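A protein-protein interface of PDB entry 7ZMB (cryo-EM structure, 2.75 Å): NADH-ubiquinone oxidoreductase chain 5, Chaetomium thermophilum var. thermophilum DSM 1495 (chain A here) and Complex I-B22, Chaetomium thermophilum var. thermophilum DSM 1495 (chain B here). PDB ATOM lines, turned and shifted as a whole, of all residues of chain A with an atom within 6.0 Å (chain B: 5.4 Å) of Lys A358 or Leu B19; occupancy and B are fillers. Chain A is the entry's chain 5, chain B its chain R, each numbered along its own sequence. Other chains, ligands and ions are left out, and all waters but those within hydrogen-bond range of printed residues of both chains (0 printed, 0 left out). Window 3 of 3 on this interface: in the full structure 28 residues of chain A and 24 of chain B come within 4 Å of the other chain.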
ATOM      1  N   VAL A 350      16.023 -38.771 -29.307  1.00  0.00           N
ATOM      2  CA  VAL A 350      14.794 -38.721 -28.525  1.00  0.00           C
ATOM      3  C   VAL A 350      13.707 -39.429 -29.318  1.00  0.00           C
ATOM      4  O   VAL A 350      13.922 -39.821 -30.470  1.00  0.00           O
ATOM      5  CB  VAL A 350      14.389 -37.274 -28.196  1.00  0.00           C
ATOM      6  CG1 VAL A 350      15.462 -36.605 -27.354  1.00  0.00           C
ATOM      7  CG2 VAL A 350      14.130 -36.498 -29.471  1.00  0.00           C
ATOM      8  N   ASN A 353      11.031 -36.096 -30.691  1.00  0.00           N
ATOM      9  CA  ASN A 353      10.556 -34.847 -30.125  1.00  0.00           C
ATOM     10  C   ASN A 353      11.290 -33.687 -30.785  1.00  0.00           C
ATOM     11  O   ASN A 353      12.437 -33.816 -31.212  1.00  0.00           O
ATOM     12  CB  ASN A 353      10.764 -34.825 -28.608  1.00  0.00           C
ATOM     13  CG  ASN A 353      10.238 -33.558 -27.957  1.00  0.00           C
ATOM     14  OD1 ASN A 353      10.653 -32.448 -28.290  1.00  0.00           O
ATOM     15  ND2 ASN A 353       9.310 -33.723 -27.023  1.00  0.00           N
ATOM     16  N   ASP A 355      10.631 -30.210 -29.424  1.00  0.00           N
ATOM     17  CA  ASP A 355      10.483 -29.039 -28.574  1.00  0.00           C
ATOM     18  C   ASP A 355      11.714 -28.838 -27.700  1.00  0.00           C
ATOM     19  O   ASP A 355      12.255 -29.791 -27.133  1.00  0.00           O
ATOM     20  CB  ASP A 355       9.238 -29.166 -27.697  1.00  0.00           C
ATOM     21  CG  ASP A 355       8.710 -27.822 -27.237  1.00  0.00           C
ATOM     22  OD1 ASP A 355       9.525 -26.898 -27.041  1.00  0.00           O
ATOM     23  OD2 ASP A 355       7.479 -27.688 -27.075  1.00  0.00           O
ATOM     24  N   PHE A 356      12.150 -27.580 -27.592  1.00  0.00           N
ATOM     25  CA  PHE A 356      13.256 -27.245 -26.705  1.00  0.00           C
ATOM     26  C   PHE A 356      12.880 -27.370 -25.237  1.00  0.00           C
ATOM     27  O   PHE A 356      13.770 -27.529 -24.395  1.00  0.00           O
ATOM     28  CB  PHE A 356      13.744 -25.824 -26.978  1.00  0.00           C
ATOM     29  CG  PHE A 356      14.474 -25.672 -28.276  1.00  0.00           C
ATOM     30  CD1 PHE A 356      15.824 -25.956 -28.360  1.00  0.00           C
ATOM     31  CD2 PHE A 356      13.814 -25.235 -29.407  1.00  0.00           C
ATOM     32  CE1 PHE A 356      16.502 -25.813 -29.551  1.00  0.00           C
ATOM     33  CE2 PHE A 356      14.485 -25.088 -30.599  1.00  0.00           C
ATOM     34  CZ  PHE A 356      15.831 -25.379 -30.672  1.00  0.00           C
ATOM     35  N   ARG A 357      11.588 -27.295 -24.913  1.00  0.00           N
ATOM     36  CA  ARG A 357      11.160 -27.339 -23.521  1.00  0.00           C
ATOM     37  C   ARG A 357      11.461 -28.676 -22.863  1.00  0.00           C
ATOM     38  O   ARG A 357      11.487 -28.753 -21.629  1.00  0.00           O
ATOM     39  CB  ARG A 357       9.667 -27.035 -23.428  1.00  0.00           C
ATOM     40  CG  ARG A 357       9.283 -25.715 -24.072  1.00  0.00           C
ATOM     41  CD  ARG A 357       8.051 -25.111 -23.424  1.00  0.00           C
ATOM     42  NE  ARG A 357       7.372 -24.188 -24.329  1.00  0.00           N
ATOM     43  CZ  ARG A 357       6.550 -24.571 -25.302  1.00  0.00           C
ATOM     44  NH1 ARG A 357       5.976 -23.674 -26.082  1.00  0.00           N
ATOM     45  NH2 ARG A 357       6.315 -25.853 -25.501  1.00  0.00           N
ATOM     46  N   LYS A 358      11.685 -29.725 -23.647  1.00  0.00           N
ATOM     47  CA  LYS A 358      12.023 -31.045 -23.138  1.00  0.00           C
ATOM     48  C   LYS A 358      13.339 -31.534 -23.718  1.00  0.00           C
ATOM     49  O   LYS A 358      13.517 -32.720 -23.997  1.00  0.00           O
ATOM     50  CB  LYS A 358      10.900 -32.044 -23.406  1.00  0.00           C
ATOM     51  CG  LYS A 358       9.733 -31.979 -22.416  1.00  0.00           C
ATOM     52  CD  LYS A 358       8.845 -30.761 -22.593  1.00  0.00           C
ATOM     53  CE  LYS A 358       7.657 -30.816 -21.642  1.00  0.00           C
ATOM     54  NZ  LYS A 358       6.817 -29.587 -21.694  1.00  0.00           N
ATOM     55  N   PHE A 359      14.282 -30.615 -23.902  1.00  0.00           N
ATOM     56  CA  PHE A 359      15.630 -30.932 -24.340  1.00  0.00           C
ATOM     57  C   PHE A 359      16.626 -30.435 -23.302  1.00  0.00           C
ATOM     58  O   PHE A 359      16.404 -29.412 -22.647  1.00  0.00           O
ATOM     59  CB  PHE A 359      15.949 -30.298 -25.700  1.00  0.00           C
ATOM     60  CG  PHE A 359      15.337 -31.018 -26.867  1.00  0.00           C
ATOM     61  CD1 PHE A 359      14.802 -32.284 -26.718  1.00  0.00           C
ATOM     62  CD2 PHE A 359      15.309 -30.430 -28.119  1.00  0.00           C
ATOM     63  CE1 PHE A 359      14.241 -32.945 -27.792  1.00  0.00           C
ATOM     64  CE2 PHE A 359      14.752 -31.086 -29.197  1.00  0.00           C
ATOM     65  CZ  PHE A 359      14.216 -32.345 -29.034  1.00  0.00           C
ATOM     66  N   GLY A 360      17.724 -31.163 -23.156  1.00  0.00           N
ATOM     67  CA  GLY A 360      18.757 -30.770 -22.219  1.00  0.00           C
ATOM     68  C   GLY A 360      19.793 -31.858 -22.082  1.00  0.00           C
ATOM     69  O   GLY A 360      19.601 -32.997 -22.515  1.00  0.00           O
ATOM     70  N   ASN A 438      15.583 -31.721 -19.497  1.00  0.00           N
ATOM     71  CA  ASN A 438      14.196 -31.294 -19.373  1.00  0.00           C
ATOM     72  C   ASN A 438      13.215 -32.304 -19.954  1.00  0.00           C
ATOM     73  O   ASN A 438      12.011 -32.029 -19.986  1.00  0.00           O
ATOM     74  CB  ASN A 438      13.992 -29.928 -20.036  1.00  0.00           C
ATOM     75  CG  ASN A 438      14.436 -28.784 -19.151  1.00  0.00           C
ATOM     76  OD1 ASN A 438      15.557 -28.776 -18.642  1.00  0.00           O
ATOM     77  ND2 ASN A 438      13.555 -27.809 -18.954  1.00  0.00           N
ATOM     78  N   GLY A 439      13.691 -33.455 -20.415  1.00  0.00           N
ATOM     79  CA  GLY A 439      12.822 -34.506 -20.884  1.00  0.00           C
ATOM     80  C   GLY A 439      12.550 -35.543 -19.813  1.00  0.00           C
ATOM     81  O   GLY A 439      12.846 -35.343 -18.632  1.00  0.00           O
ATOM     82  N   PRO A 440      11.974 -36.672 -20.208  1.00  0.00           N
ATOM     83  CA  PRO A 440      11.707 -37.760 -19.262  1.00  0.00           C
ATOM     84  C   PRO A 440      12.976 -38.558 -18.978  1.00  0.00           C
ATOM     85  O   PRO A 440      14.042 -38.302 -19.534  1.00  0.00           O
ATOM     86  CB  PRO A 440      10.658 -38.620 -19.974  1.00  0.00           C
ATOM     87  CG  PRO A 440      10.574 -38.124 -21.372  1.00  0.00           C
ATOM     88  CD  PRO A 440      11.484 -36.959 -21.564  1.00  0.00           C
ATOM     89  N   TYR A 443      15.176 -40.659 -21.826  1.00  0.00           N
ATOM     90  CA  TYR A 443      16.144 -40.001 -22.693  1.00  0.00           C
ATOM     91  C   TYR A 443      17.561 -40.076 -22.143  1.00  0.00           C
ATOM     92  O   TYR A 443      18.516 -39.973 -22.919  1.00  0.00           O
ATOM     93  CB  TYR A 443      15.758 -38.536 -22.906  1.00  0.00           C
ATOM     94  CG  TYR A 443      14.545 -38.329 -23.786  1.00  0.00           C
ATOM     95  CD1 TYR A 443      13.930 -39.399 -24.419  1.00  0.00           C
ATOM     96  CD2 TYR A 443      14.021 -37.059 -23.989  1.00  0.00           C
ATOM     97  CE1 TYR A 443      12.824 -39.213 -25.223  1.00  0.00           C
ATOM     98  CE2 TYR A 443      12.916 -36.864 -24.792  1.00  0.00           C
ATOM     99  CZ  TYR A 443      12.321 -37.944 -25.407  1.00  0.00           C
ATOM    100  OH  TYR A 443      11.220 -37.758 -26.209  1.00  0.00           O
ATOM    101  N   TYR A 444      17.724 -40.256 -20.831  1.00  0.00           N
ATOM    102  CA  TYR A 444      19.039 -40.206 -20.210  1.00  0.00           C
ATOM    103  C   TYR A 444      19.362 -41.388 -19.309  1.00  0.00           C
ATOM    104  O   TYR A 444      20.494 -41.465 -18.820  1.00  0.00           O
ATOM    105  CB  TYR A 444      19.192 -38.922 -19.385  1.00  0.00           C
ATOM    106  CG  TYR A 444      18.728 -37.679 -20.096  1.00  0.00           C
ATOM    107  CD1 TYR A 444      19.573 -36.995 -20.955  1.00  0.00           C
ATOM    108  CD2 TYR A 444      17.445 -37.188 -19.907  1.00  0.00           C
ATOM    109  CE1 TYR A 444      19.155 -35.860 -21.605  1.00  0.00           C
ATOM    110  CE2 TYR A 444      17.017 -36.051 -20.554  1.00  0.00           C
ATOM    111  CZ  TYR A 444      17.876 -35.390 -21.401  1.00  0.00           C
ATOM    112  OH  TYR A 444      17.455 -34.254 -22.051  1.00  0.00           O
ATOM    113  N   LEU B  15      -0.749 -25.460 -13.682  1.00  0.00           N
ATOM    114  CA  LEU B  15       0.682 -25.692 -13.547  1.00  0.00           C
ATOM    115  C   LEU B  15       1.298 -26.114 -14.873  1.00  0.00           C
ATOM    116  O   LEU B  15       2.474 -25.830 -15.126  1.00  0.00           O
ATOM    117  CB  LEU B  15       0.945 -26.730 -12.453  1.00  0.00           C
ATOM    118  CG  LEU B  15       0.398 -28.156 -12.573  1.00  0.00           C
ATOM    119  CD1 LEU B  15       1.299 -29.047 -13.420  1.00  0.00           C
ATOM    120  CD2 LEU B  15       0.199 -28.755 -11.192  1.00  0.00           C
ATOM    121  N   LYS B  16       0.523 -26.785 -15.728  1.00  0.00           N
ATOM    122  CA  LYS B  16       1.018 -27.136 -17.054  1.00  0.00           C
ATOM    123  C   LYS B  16       1.275 -25.890 -17.887  1.00  0.00           C
ATOM    124  O   LYS B  16       2.258 -25.827 -18.635  1.00  0.00           O
ATOM    125  CB  LYS B  16       0.024 -28.060 -17.760  1.00  0.00           C
ATOM    126  CG  LYS B  16       0.491 -28.541 -19.123  1.00  0.00           C
ATOM    127  CD  LYS B  16      -0.500 -29.514 -19.735  1.00  0.00           C
ATOM    128  CE  LYS B  16       0.004 -30.043 -21.066  1.00  0.00           C
ATOM    129  NZ  LYS B  16       0.035 -28.982 -22.109  1.00  0.00           N
ATOM    130  N   LEU B  17       0.400 -24.889 -17.775  1.00  0.00           N
ATOM    131  CA  LEU B  17       0.604 -23.647 -18.513  1.00  0.00           C
ATOM    132  C   LEU B  17       1.867 -22.935 -18.047  1.00  0.00           C
ATOM    133  O   LEU B  17       2.609 -22.375 -18.862  1.00  0.00           O
ATOM    134  CB  LEU B  17      -0.624 -22.745 -18.371  1.00  0.00           C
ATOM    135  CG  LEU B  17      -0.691 -21.467 -19.211  1.00  0.00           C
ATOM    136  CD1 LEU B  17      -2.135 -21.079 -19.457  1.00  0.00           C
ATOM    137  CD2 LEU B  17       0.033 -20.311 -18.545  1.00  0.00           C
ATOM    138  N   ALA B  18       2.120 -22.937 -16.737  1.00  0.00           N
ATOM    139  CA  ALA B  18       3.305 -22.264 -16.216  1.00  0.00           C
ATOM    140  C   ALA B  18       4.581 -22.900 -16.748  1.00  0.00           C
ATOM    141  O   ALA B  18       5.546 -22.199 -17.071  1.00  0.00           O
ATOM    142  CB  ALA B  18       3.291 -22.287 -14.687  1.00  0.00           C
ATOM    143  N   LEU B  19       4.601 -24.232 -16.850  1.00  0.00           N
ATOM    144  CA  LEU B  19       5.807 -24.923 -17.288  1.00  0.00           C
ATOM    145  C   LEU B  19       6.134 -24.594 -18.739  1.00  0.00           C
ATOM    146  O   LEU B  19       7.309 -24.526 -19.116  1.00  0.00           O
ATOM    147  CB  LEU B  19       5.638 -26.430 -17.086  1.00  0.00           C
ATOM    148  CG  LEU B  19       6.822 -27.378 -17.301  1.00  0.00           C
ATOM    149  CD1 LEU B  19       6.634 -28.619 -16.451  1.00  0.00           C
ATOM    150  CD2 LEU B  19       6.970 -27.779 -18.759  1.00  0.00           C
ATOM    151  N   ASP B  20       5.111 -24.384 -19.567  1.00  0.00           N
ATOM    152  CA  ASP B  20       5.350 -24.098 -20.974  1.00  0.00           C
ATOM    153  C   ASP B  20       5.828 -22.674 -21.208  1.00  0.00           C
ATOM    154  O   ASP B  20       6.355 -22.383 -22.284  1.00  0.00           O
ATOM    155  CB  ASP B  20       4.090 -24.372 -21.793  1.00  0.00           C
ATOM    156  CG  ASP B  20       3.982 -25.819 -22.203  1.00  0.00           C
ATOM    157  OD1 ASP B  20       4.959 -26.557 -21.977  1.00  0.00           O
ATOM    158  OD2 ASP B  20       2.931 -26.223 -22.741  1.00  0.00           O
ATOM    159  N   TRP B  21       5.656 -21.791 -20.226  1.00  0.00           N
ATOM    160  CA  TRP B  21       6.235 -20.451 -20.278  1.00  0.00           C
ATOM    161  C   TRP B  21       7.667 -20.425 -19.763  1.00  0.00           C
ATOM    162  O   TRP B  21       8.515 -19.727 -20.329  1.00  0.00           O
ATOM    163  CB  TRP B  21       5.356 -19.486 -19.489  1.00  0.00           C
ATOM    164  CG  TRP B  21       4.431 -18.694 -20.332  1.00  0.00           C
ATOM    165  CD1 TRP B  21       3.074 -18.671 -20.272  1.00  0.00           C
ATOM    166  CD2 TRP B  21       4.808 -17.697 -21.287  1.00  0.00           C
ATOM    167  NE1 TRP B  21       2.575 -17.772 -21.184  1.00  0.00           N
ATOM    168  CE2 TRP B  21       3.623 -17.154 -21.814  1.00  0.00           C
ATOM    169  CE3 TRP B  21       6.034 -17.233 -21.767  1.00  0.00           C
ATOM    170  CZ2 TRP B  21       3.629 -16.172 -22.800  1.00  0.00           C
ATOM    171  CZ3 TRP B  21       6.035 -16.255 -22.738  1.00  0.00           C
ATOM    172  CH2 TRP B  21       4.842 -15.737 -23.247  1.00  0.00           C
ATOM    173  N   THR B  22       7.962 -21.181 -18.709  1.00  0.00           N
ATOM    174  CA  THR B  22       9.285 -21.211 -18.092  1.00  0.00           C
ATOM    175  C   THR B  22       9.965 -22.525 -18.458  1.00  0.00           C
ATOM    176  O   THR B  22       9.608 -23.582 -17.926  1.00  0.00           O
ATOM    177  CB  THR B  22       9.179 -21.057 -16.577  1.00  0.00           C
ATOM    178  OG1 THR B  22       8.425 -22.148 -16.039  1.00  0.00           O
ATOM    179  CG2 THR B  22       8.483 -19.756 -16.227  1.00  0.00           C
ATOM    180  N   VAL B  23      10.952 -22.457 -19.351  1.00  0.00           N
ATOM    181  CA  VAL B  23      11.601 -23.676 -19.826  1.00  0.00           C
ATOM    182  C   VAL B  23      12.396 -24.343 -18.708  1.00  0.00           C
ATOM    183  O   VAL B  23      12.377 -25.572 -18.569  1.00  0.00           O
ATOM    184  CB  VAL B  23      12.469 -23.375 -21.062  1.00  0.00           C
ATOM    185  CG1 VAL B  23      13.629 -22.449 -20.718  1.00  0.00           C
ATOM    186  CG2 VAL B  23      12.980 -24.671 -21.673  1.00  0.00           C
ATOM    187  N   ARG B  25      12.505 -25.742 -15.505  1.00  0.00           N
ATOM    188  CA  ARG B  25      11.373 -26.160 -14.691  1.00  0.00           C
ATOM    189  C   ARG B  25      11.699 -26.280 -13.211  1.00  0.00           C
ATOM    190  O   ARG B  25      10.801 -26.599 -12.424  1.00  0.00           O
ATOM    191  CB  ARG B  25      10.807 -27.486 -15.204  1.00  0.00           C
ATOM    192  CG  ARG B  25      11.643 -28.704 -14.890  1.00  0.00           C
ATOM    193  CD  ARG B  25      11.183 -29.876 -15.735  1.00  0.00           C
ATOM    194  NE  ARG B  25       9.784 -30.215 -15.492  1.00  0.00           N
ATOM    195  CZ  ARG B  25       9.370 -31.386 -15.021  1.00  0.00           C
ATOM    196  NH1 ARG B  25      10.250 -32.336 -14.740  1.00  0.00           N
ATOM    197  NH2 ARG B  25       8.078 -31.608 -14.829  1.00  0.00           N
ATOM    198  N   TRP B  28       9.845 -23.574 -12.403  1.00  0.00           N
ATOM    199  CA  TRP B  28       8.470 -24.058 -12.375  1.00  0.00           C
ATOM    200  C   TRP B  28       8.205 -24.919 -11.150  1.00  0.00           C
ATOM    201  O   TRP B  28       7.062 -25.002 -10.688  1.00  0.00           O
ATOM    202  CB  TRP B  28       8.164 -24.843 -13.650  1.00  0.00           C
ATOM    203  CG  TRP B  28       6.896 -25.632 -13.598  1.00  0.00           C
ATOM    204  CD1 TRP B  28       5.639 -25.174 -13.836  1.00  0.00           C
ATOM    205  CD2 TRP B  28       6.764 -27.021 -13.287  1.00  0.00           C
ATOM    206  NE1 TRP B  28       4.729 -26.191 -13.699  1.00  0.00           N
ATOM    207  CE2 TRP B  28       5.396 -27.337 -13.359  1.00  0.00           C
ATOM    208  CE3 TRP B  28       7.671 -28.031 -12.955  1.00  0.00           C
ATOM    209  CZ2 TRP B  28       4.910 -28.619 -13.110  1.00  0.00           C
ATOM    210  CZ3 TRP B  28       7.188 -29.302 -12.708  1.00  0.00           C
ATOM    211  CH2 TRP B  28       5.821 -29.585 -12.788  1.00  0.00           C
ATOM    212  N   TYR B  71       3.401 -26.820 -25.190  1.00  0.00           N
ATOM    213  CA  TYR B  71       4.036 -28.085 -25.524  1.00  0.00           C
ATOM    214  C   TYR B  71       2.997 -29.180 -25.724  1.00  0.00           C
ATOM    215  O   TYR B  71       2.003 -29.259 -24.998  1.00  0.00           O
ATOM    216  CB  TYR B  71       5.015 -28.501 -24.426  1.00  0.00           C
ATOM    217  CG  TYR B  71       5.510 -29.918 -24.555  1.00  0.00           C
ATOM    218  CD1 TYR B  71       6.642 -30.205 -25.294  1.00  0.00           C
ATOM    219  CD2 TYR B  71       4.842 -30.971 -23.944  1.00  0.00           C
ATOM    220  CE1 TYR B  71       7.096 -31.501 -25.427  1.00  0.00           C
ATOM    221  CE2 TYR B  71       5.285 -32.262 -24.069  1.00  0.00           C
ATOM    222  CZ  TYR B  71       6.415 -32.525 -24.808  1.00  0.00           C
ATOM    223  OH  TYR B  71       6.866 -33.818 -24.934  1.00  0.00           O
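NH2 of Arg A357 is in salt-bridge range of OD1 of Asp B20 (3.8 Å). The side-chain carboxylate (OD1) of Asp B20 lies within salt-bridge range of the side-chain amino group (NZ) of Lys A358 (3.6 Å). The side-chain amide nitrogen of Asn A438 is in hydrogen-bond range of the backbone carbonyl oxygen of Val B23, at 2.6 Å. The side-chain amide nitrogen of Asn A353 is in hydrogen-bond range of the side-chain hydroxyl of Tyr B71 (3.2 Å). N of Tyr B71 sits close to NH2 of Arg A357.
OD2 of Asp B20 lies within hydrogen-bond range of N of Tyr B71, 2.6 Å away. The backbone NH (N) of Asp A355 is in hydrogen-bond range of the side-chain amide oxygen (OD1) of Asn A353 (2.5 Å). OD2 of Asp A355 lies within salt-bridge range of NH2 of Arg A357.
Tyr B71 touches Asp A355 (CD1 to OD2, 3.2 Å). CA of Arg A357 touches CG2 of Val B23 (3.7 Å). NZ of Lys A358 touches CD2 of Leu B19, at 3.5 Å. Tyr B71 touches Lys A358 (CG to NZ, 3.2 Å).
Lys A358 touches just these residues of chain B: Leu B19, Asp B20 and Tyr B71. Printed residues of chain B within 4 Å of Asn A438: Val B23 (2.6 Å). Ala B18 touches none of the printed residues of chain A. Trp B21 touches none of the printed residues of chain A. Of the printed residues of chain A, Val B23 touches Arg A357 (3.7 Å) and Asn A438 (2.6 Å). The nearest printed residue of chain B that does not touch Lys A358 is Val B23 (5.6 Å). The nearest residue of chain A that does not touch Leu B19 is Arg A357 (4.4 Å).
Of the 13 printed residues of chain A, 5 touch a printed residue of chain B. Hydrophobic or aromatic side chains of chain B that line the printed part of chain A: Leu B19, Val B23 and Tyr B71. Among the printed residues, 9 pairs touch across the chains.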
